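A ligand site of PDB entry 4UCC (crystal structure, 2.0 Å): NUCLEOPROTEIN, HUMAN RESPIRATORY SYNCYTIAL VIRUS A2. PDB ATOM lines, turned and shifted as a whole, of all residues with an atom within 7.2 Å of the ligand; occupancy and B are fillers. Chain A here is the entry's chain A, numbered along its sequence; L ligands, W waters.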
ATOM      1  N   HIS A  16       7.535  27.072  18.623  1.00  0.00           N
ATOM      2  CA  HIS A  16       8.162  27.309  17.322  1.00  0.00           C
ATOM      3  C   HIS A  16       8.755  28.710  17.230  1.00  0.00           C
ATOM      4  O   HIS A  16       9.886  28.857  16.776  1.00  0.00           O
ATOM      5  CB  HIS A  16       7.186  27.078  16.175  1.00  0.00           C
ATOM      6  CG  HIS A  16       7.873  27.076  14.842  1.00  0.00           C
ATOM      7  ND1 HIS A  16       8.120  25.900  14.171  1.00  0.00           N
ATOM      8  CD2 HIS A  16       8.369  28.103  14.124  1.00  0.00           C
ATOM      9  CE1 HIS A  16       8.758  26.242  13.076  1.00  0.00           C
ATOM     10  NE2 HIS A  16       8.926  27.558  12.993  1.00  0.00           N
ATOM     11  N   LYS A  19      11.986  29.065  19.365  1.00  0.00           N
ATOM     12  CA  LYS A  19      13.063  28.373  18.639  1.00  0.00           C
ATOM     13  C   LYS A  19      13.604  29.272  17.494  1.00  0.00           C
ATOM     14  O   LYS A  19      14.811  29.295  17.250  1.00  0.00           O
ATOM     15  CB  LYS A  19      12.509  27.051  18.081  1.00  0.00           C
ATOM     16  CG  LYS A  19      13.529  26.066  17.586  1.00  0.00           C
ATOM     17  CD  LYS A  19      12.904  24.665  17.471  1.00  0.00           C
ATOM     18  CE  LYS A  19      12.470  24.113  18.817  1.00  0.00           C
ATOM     19  NZ  LYS A  19      11.304  23.189  18.724  1.00  0.00           N
ATOM     20  N   GLY A  22      15.682  31.774  19.160  1.00  0.00           N
ATOM     21  CA  GLY A  22      16.926  31.102  19.547  1.00  0.00           C
ATOM     22  C   GLY A  22      17.884  30.856  18.396  1.00  0.00           C
ATOM     23  O   GLY A  22      19.106  30.978  18.554  1.00  0.00           O
ATOM     24  N   MET A  23      17.327  30.563  17.220  1.00  0.00           N
ATOM     25  CA  MET A  23      18.140  30.397  15.994  1.00  0.00           C
ATOM     26  C   MET A  23      18.871  31.683  15.648  1.00  0.00           C
ATOM     27  O   MET A  23      20.058  31.632  15.291  1.00  0.00           O
ATOM     28  CB  MET A  23      17.285  29.905  14.811  1.00  0.00           C
ATOM     29  CG  MET A  23      16.880  28.468  14.956  1.00  0.00           C
ATOM     30  SD  MET A  23      16.078  27.820  13.477  1.00  0.00           S
ATOM     31  CE  MET A  23      14.450  28.347  13.650  1.00  0.00           C
ATOM     32  N   ILE A  26      21.800  32.314  18.302  1.00  0.00           N
ATOM     33  CA  ILE A  26      23.045  31.543  18.133  1.00  0.00           C
ATOM     34  C   ILE A  26      23.788  31.917  16.830  1.00  0.00           C
ATOM     35  O   ILE A  26      24.888  31.401  16.584  1.00  0.00           O
ATOM     36  CB  ILE A  26      22.871  29.999  18.290  1.00  0.00           C
ATOM     37  CG1 ILE A  26      22.102  29.375  17.097  1.00  0.00           C
ATOM     38  CG2 ILE A  26      22.262  29.613  19.627  1.00  0.00           C
ATOM     39  CD1 ILE A  26      22.539  27.886  16.824  1.00  0.00           C
ATOM     40  N   PHE A  84      11.912  21.441   6.121  1.00  0.00           N
ATOM     41  CA  PHE A  84      11.935  22.552   7.085  1.00  0.00           C
ATOM     42  C   PHE A  84      10.565  22.791   7.669  1.00  0.00           C
ATOM     43  O   PHE A  84       9.583  22.813   6.932  1.00  0.00           O
ATOM     44  CB  PHE A  84      12.406  23.859   6.424  1.00  0.00           C
ATOM     45  CG  PHE A  84      13.828  23.877   5.940  1.00  0.00           C
ATOM     46  CD1 PHE A  84      14.153  23.421   4.667  1.00  0.00           C
ATOM     47  CD2 PHE A  84      14.843  24.379   6.732  1.00  0.00           C
ATOM     48  CE1 PHE A  84      15.472  23.438   4.213  1.00  0.00           C
ATOM     49  CE2 PHE A  84      16.158  24.400   6.285  1.00  0.00           C
ATOM     50  CZ  PHE A  84      16.469  23.921   5.029  1.00  0.00           C
ATOM     51  N   GLU A  85      10.505  23.018   8.987  1.00  0.00           N
ATOM     52  CA  GLU A  85       9.253  23.375   9.617  1.00  0.00           C
ATOM     53  C   GLU A  85       9.182  24.901   9.629  1.00  0.00           C
ATOM     54  O   GLU A  85      10.100  25.580  10.109  1.00  0.00           O
ATOM     55  CB  GLU A  85       9.084  22.734  11.000  1.00  0.00           C
ATOM     56  CG  GLU A  85       8.684  21.266  10.911  1.00  0.00           C
ATOM     57  CD  GLU A  85       7.340  20.897  11.518  1.00  0.00           C
ATOM     58  OE1 GLU A  85       7.193  21.020  12.762  1.00  0.00           O
ATOM     59  OE2 GLU A  85       6.460  20.427  10.764  1.00  0.00           O
ATOM     60  N   ILE A 100      16.947  31.756   7.890  1.00  0.00           N
ATOM     61  CA  ILE A 100      17.310  31.914   9.300  1.00  0.00           C
ATOM     62  C   ILE A 100      17.778  30.525   9.867  1.00  0.00           C
ATOM     63  O   ILE A 100      18.814  30.461  10.530  1.00  0.00           O
ATOM     64  CB  ILE A 100      16.145  32.534  10.125  1.00  0.00           C
ATOM     65  CG1 ILE A 100      15.983  34.043   9.776  1.00  0.00           C
ATOM     66  CG2 ILE A 100      16.360  32.303  11.648  1.00  0.00           C
ATOM     67  CD1 ILE A 100      14.709  34.734  10.324  1.00  0.00           C
ATOM     68  N   GLU A 101      17.031  29.428   9.537  1.00  0.00           N
ATOM     69  CA  GLU A 101      17.428  28.085  10.002  1.00  0.00           C
ATOM     70  C   GLU A 101      18.779  27.664   9.411  1.00  0.00           C
ATOM     71  O   GLU A 101      19.595  27.126  10.150  1.00  0.00           O
ATOM     72  CB  GLU A 101      16.356  27.031   9.738  1.00  0.00           C
ATOM     73  CG  GLU A 101      16.749  25.621  10.159  1.00  0.00           C
ATOM     74  CD  GLU A 101      15.649  24.587  10.034  1.00  0.00           C
ATOM     75  OE1 GLU A 101      14.505  24.941  10.387  1.00  0.00           O
ATOM     76  OE2 GLU A 101      15.921  23.396   9.727  1.00  0.00           O
ATOM     77  N   ILE A 102      19.011  27.901   8.107  1.00  0.00           N
ATOM     78  CA  ILE A 102      20.275  27.585   7.412  1.00  0.00           C
ATOM     79  C   ILE A 102      21.470  28.273   8.112  1.00  0.00           C
ATOM     80  O   ILE A 102      22.391  27.588   8.495  1.00  0.00           O
ATOM     81  CB  ILE A 102      20.238  27.912   5.893  1.00  0.00           C
ATOM     82  CG1 ILE A 102      19.170  27.017   5.196  1.00  0.00           C
ATOM     83  CG2 ILE A 102      21.635  27.760   5.230  1.00  0.00           C
ATOM     84  CD1 ILE A 102      18.834  27.409   3.672  1.00  0.00           C
ATOM     85  N   GLU A 103      21.433  29.615   8.238  1.00  0.00           N
ATOM     86  CA  GLU A 103      22.486  30.399   8.882  1.00  0.00           C
ATOM     87  C   GLU A 103      22.750  29.955  10.340  1.00  0.00           C
ATOM     88  O   GLU A 103      23.910  29.858  10.751  1.00  0.00           O
ATOM     89  CB  GLU A 103      22.200  31.906   8.778  1.00  0.00           C
ATOM     90  CG  GLU A 103      22.267  32.462   7.367  1.00  0.00           C
ATOM     91  CD  GLU A 103      23.517  32.174   6.535  1.00  0.00           C
ATOM     92  OE1 GLU A 103      24.643  32.227   7.102  1.00  0.00           O
ATOM     93  OE2 GLU A 103      23.371  31.906   5.321  1.00  0.00           O
ATOM     94  N   SER A 104      21.671  29.627  11.081  1.00  0.00           N
ATOM     95  CA  SER A 104      21.764  29.145  12.446  1.00  0.00           C
ATOM     96  C   SER A 104      22.469  27.782  12.543  1.00  0.00           C
ATOM     97  O   SER A 104      23.315  27.585  13.417  1.00  0.00           O
ATOM     98  CB  SER A 104      20.371  29.081  13.058  1.00  0.00           C
ATOM     99  OG  SER A 104      20.506  28.763  14.427  1.00  0.00           O
ATOM    100  N   ARG A 105      22.147  26.871  11.619  1.00  0.00           N
ATOM    101  CA  ARG A 105      22.763  25.533  11.563  1.00  0.00           C
ATOM    102  C   ARG A 105      24.253  25.631  11.231  1.00  0.00           C
ATOM    103  O   ARG A 105      25.018  24.804  11.733  1.00  0.00           O
ATOM    104  CB  ARG A 105      22.052  24.646  10.539  1.00  0.00           C
ATOM    105  CG  ARG A 105      20.717  24.098  11.040  1.00  0.00           C
ATOM    106  CD  ARG A 105      20.114  23.241   9.950  1.00  0.00           C
ATOM    107  NE  ARG A 105      18.825  22.687  10.342  1.00  0.00           N
ATOM    108  CZ  ARG A 105      18.654  21.525  10.977  1.00  0.00           C
ATOM    109  NH1 ARG A 105      19.699  20.762  11.282  1.00  0.00           N
ATOM    110  NH2 ARG A 105      17.433  21.129  11.315  1.00  0.00           N
ATOM    111  N   LYS A 106      24.668  26.649  10.432  1.00  0.00           N
ATOM    112  CA  LYS A 106      26.094  26.906  10.120  1.00  0.00           C
ATOM    113  C   LYS A 106      26.817  27.360  11.424  1.00  0.00           C
ATOM    114  O   LYS A 106      27.935  26.927  11.665  1.00  0.00           O
ATOM    115  CB  LYS A 106      26.252  28.020   9.071  1.00  0.00           C
ATOM    116  CG  LYS A 106      25.903  27.633   7.647  1.00  0.00           C
ATOM    117  CD  LYS A 106      26.286  28.787   6.685  1.00  0.00           C
ATOM    118  CE  LYS A 106      25.556  28.714   5.358  1.00  0.00           C
ATOM    119  NZ  LYS A 106      25.851  29.915   4.522  1.00  0.00           N
ATOM    120  N   SER A 107      26.206  28.238  12.225  1.00  0.00           N
ATOM    121  CA  SER A 107      26.797  28.704  13.496  1.00  0.00           C
ATOM    122  C   SER A 107      26.846  27.543  14.513  1.00  0.00           C
ATOM    123  O   SER A 107      27.820  27.410  15.239  1.00  0.00           O
ATOM    124  CB  SER A 107      26.035  29.899  14.060  1.00  0.00           C
ATOM    125  OG  SER A 107      26.449  31.089  13.388  1.00  0.00           O
ATOM    126  N   TYR A 108      25.819  26.660  14.492  1.00  0.00           N
ATOM    127  CA  TYR A 108      25.767  25.525  15.411  1.00  0.00           C
ATOM    128  C   TYR A 108      26.886  24.536  15.115  1.00  0.00           C
ATOM    129  O   TYR A 108      27.483  24.035  16.050  1.00  0.00           O
ATOM    130  CB  TYR A 108      24.392  24.836  15.354  1.00  0.00           C
ATOM    131  CG  TYR A 108      24.248  23.709  16.341  1.00  0.00           C
ATOM    132  CD1 TYR A 108      23.837  23.952  17.648  1.00  0.00           C
ATOM    133  CD2 TYR A 108      24.497  22.395  15.970  1.00  0.00           C
ATOM    134  CE1 TYR A 108      23.720  22.919  18.578  1.00  0.00           C
ATOM    135  CE2 TYR A 108      24.370  21.341  16.892  1.00  0.00           C
ATOM    136  CZ  TYR A 108      23.973  21.607  18.182  1.00  0.00           C
ATOM    137  OH  TYR A 108      23.793  20.579  19.061  1.00  0.00           O
ATOM    138  N   LYS A 109      27.175  24.245  13.838  1.00  0.00           N
ATOM    139  CA  LYS A 109      28.233  23.324  13.483  1.00  0.00           C
ATOM    140  C   LYS A 109      29.612  23.858  13.926  1.00  0.00           C
ATOM    141  O   LYS A 109      30.481  23.089  14.372  1.00  0.00           O
ATOM    142  CB  LYS A 109      28.209  22.978  11.976  1.00  0.00           C
ATOM    143  CG  LYS A 109      29.115  21.776  11.614  1.00  0.00           C
ATOM    144  CD  LYS A 109      29.126  21.481  10.099  1.00  0.00           C
ATOM    145  CE  LYS A 109      30.512  21.067   9.639  1.00  0.00           C
ATOM    146  NZ  LYS A 109      30.543  20.675   8.186  1.00  0.00           N
ATOM    147  N   LEU A 112      29.904  23.207  17.622  1.00  0.00           N
ATOM    148  CA  LEU A 112      30.263  21.811  17.876  1.00  0.00           C
ATOM    149  C   LEU A 112      31.754  21.653  17.713  1.00  0.00           C
ATOM    150  O   LEU A 112      32.411  21.065  18.575  1.00  0.00           O
ATOM    151  CB  LEU A 112      29.546  20.837  16.918  1.00  0.00           C
ATOM    152  CG  LEU A 112      28.043  20.642  17.103  1.00  0.00           C
ATOM    153  CD1 LEU A 112      27.516  19.767  16.002  1.00  0.00           C
ATOM    154  CD2 LEU A 112      27.716  19.981  18.429  1.00  0.00           C
ATOM    155  N   GLU A 117      29.520  18.851  22.049  1.00  0.00           N
ATOM    156  CA  GLU A 117      28.070  19.087  22.221  1.00  0.00           C
ATOM    157  C   GLU A 117      27.787  20.286  23.100  1.00  0.00           C
ATOM    158  O   GLU A 117      28.493  20.543  24.078  1.00  0.00           O
ATOM    159  CB  GLU A 117      27.312  17.843  22.708  1.00  0.00           C
ATOM    160  CG  GLU A 117      26.913  16.895  21.580  1.00  0.00           C
ATOM    161  CD  GLU A 117      25.907  17.419  20.559  1.00  0.00           C
ATOM    162  OE1 GLU A 117      25.255  18.451  20.828  1.00  0.00           O
ATOM    163  OE2 GLU A 117      25.796  16.785  19.477  1.00  0.00           O
ATOM    164  N   ARG A 123      21.939  26.549  23.465  1.00  0.00           N
ATOM    165  CA  ARG A 123      21.221  26.080  22.261  1.00  0.00           C
ATOM    166  C   ARG A 123      20.146  27.066  21.824  1.00  0.00           C
ATOM    167  O   ARG A 123      19.693  27.898  22.615  1.00  0.00           O
ATOM    168  CB  ARG A 123      20.582  24.716  22.523  1.00  0.00           C
ATOM    169  CG  ARG A 123      21.576  23.547  22.640  1.00  0.00           C
ATOM    170  CD  ARG A 123      20.829  22.288  23.089  1.00  0.00           C
ATOM    171  NE  ARG A 123      19.704  21.960  22.208  1.00  0.00           N
ATOM    172  CZ  ARG A 123      19.832  21.321  21.052  1.00  0.00           C
ATOM    173  NH1 ARG A 123      21.016  20.902  20.642  1.00  0.00           N
ATOM    174  NH2 ARG A 123      18.758  21.075  20.310  1.00  0.00           N
ATOM    175  N   HIS A 124      19.702  26.927  20.560  1.00  0.00           N
ATOM    176  CA  HIS A 124      18.632  27.705  19.928  1.00  0.00           C
ATOM    177  C   HIS A 124      17.237  27.380  20.547  1.00  0.00           C
ATOM    178  O   HIS A 124      16.282  28.103  20.316  1.00  0.00           O
ATOM    179  CB  HIS A 124      18.587  27.393  18.404  1.00  0.00           C
ATOM    180  CG  HIS A 124      18.046  26.017  18.071  1.00  0.00           C
ATOM    181  ND1 HIS A 124      18.789  24.858  18.301  1.00  0.00           N
ATOM    182  CD2 HIS A 124      16.848  25.663  17.553  1.00  0.00           C
ATOM    183  CE1 HIS A 124      18.024  23.853  17.926  1.00  0.00           C
ATOM    184  NE2 HIS A 124      16.849  24.283  17.475  1.00  0.00           N
ATOM    185  N   ASP A 125      17.098  26.226  21.209  1.00  0.00           N
ATOM    186  CA  ASP A 125      15.807  25.823  21.764  1.00  0.00           C
ATOM    187  C   ASP A 125      15.707  26.000  23.299  1.00  0.00           C
ATOM    188  O   ASP A 125      14.791  25.438  23.926  1.00  0.00           O
ATOM    189  CB  ASP A 125      15.428  24.395  21.337  1.00  0.00           C
ATOM    190  CG  ASP A 125      16.460  23.321  21.655  1.00  0.00           C
ATOM    191  OD1 ASP A 125      17.457  23.637  22.328  1.00  0.00           O
ATOM    192  OD2 ASP A 125      16.251  22.172  21.247  1.00  0.00           O
HETATM  193  O1  LIG L   1      22.528  19.175  13.051  1.00  0.00           O
HETATM  194  C1  LIG L   1      22.080  20.221  13.583  1.00  0.00           C
HETATM  195  O2  LIG L   1      22.071  21.368  13.053  1.00  0.00           O
HETATM  196  C2  LIG L   1      21.489  20.061  14.991  1.00  0.00           C
HETATM  197  C3  LIG L   1      21.374  18.875  15.684  1.00  0.00           C
HETATM  198  C4  LIG L   1      20.811  19.222  16.913  1.00  0.00           C
HETATM  199  C5  LIG L   1      20.526  18.241  18.073  1.00  0.00           C
HETATM  200  O3  LIG L   1      19.655  18.601  18.911  1.00  0.00           O
HETATM  201  O4  LIG L   1      21.173  17.172  18.099  1.00  0.00           O
HETATM  202  N1  LIG L   1      20.571  20.541  16.996  1.00  0.00           N
HETATM  203  N2  LIG L   1      20.995  21.034  15.800  1.00  0.00           N
HETATM  204  C6  LIG L   1      20.820  22.467  15.546  1.00  0.00           C
HETATM  205  C7  LIG L   1      19.476  22.839  14.975  1.00  0.00           C
HETATM  206  C8  LIG L   1      18.461  21.891  14.831  1.00  0.00           C
HETATM  207  C9  LIG L   1      19.191  24.134  14.551  1.00  0.00           C
HETATM  208 CL1  LIG L   1      20.368  25.386  14.748  1.00  0.00          CL
HETATM  209  C10 LIG L   1      17.978  24.478  13.995  1.00  0.00           C
HETATM  210  C11 LIG L   1      16.993  23.511  13.891  1.00  0.00           C
HETATM  211 CL2  LIG L   1      15.432  23.949  13.261  1.00  0.00          CL
HETATM  212  C12 LIG L   1      17.224  22.220  14.307  1.00  0.00           C
HETATM  213  O   HOH W   1      23.855  18.113  17.840  1.00  0.00           O
HETATM  214  O   HOH W   2      17.273  19.726  17.450  1.00  0.00           O
HETATM  215  O   HOH W   3      24.519  22.012  12.266  1.00  0.00           O
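An oxygen (O2) of the ligand is in salt-bridge range of the guanidinium group (NH1) of Arg 105, 3.0 Å away.
An oxygen (O3) of the ligand lies within salt-bridge range of the guanidinium group (NH2) of Arg 123.
OH of Tyr 108 sits at hydrogen-bond distance from NH1 of Arg 123 (3.2 Å).
OH of Tyr 108 lies within hydrogen-bond range of OE1 of Glu 117, at 3.1 Å.
OE2 of Glu 101 lies within salt-bridge range of NE of Arg 105, 3.1 Å away.
The side-chain carboxylate (OD1) of Asp 125 lies within salt-bridge range of the guanidinium group (NE) of Arg 123 (2.8 Å).
O of Met 23 lies within hydrogen-bond range of OG of Ser 104 (3.0 Å).
SD of Met 23 touches C10 of the ligand, at 3.9 Å.
Ile 26 touches the ligand.
Glu 101 touches the ligand (OE1 to CL2, 3.2 Å).
Ser 104 touches the ligand (OG to CL1, 3.4 Å).
Tyr 108 touches the ligand.
CE1 of His 124 touches C7 of the ligand, at 3.4 Å.
Within 4 Å of the ligand: Met 23, Ile 26, Glu 101, Ser 104, Arg 105, Tyr 108, Arg 123 and His 124.
Water W3 lies within hydrogen-bond range of O2 of the ligand and O of Arg 105.
Water W1 lies within hydrogen-bond range of the side-chain hydroxyl (OH) of Tyr 108 (2.8 Å), an oxygen (O4) of the ligand (2.9 Å) and the side-chain carboxylate (OE2) of Glu 117 (2.9 Å).
Water W2 bridges an oxygen (O3) of the ligand (3.0 Å) and the guanidinium group (NH2) of Arg 123 (3.5 Å).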
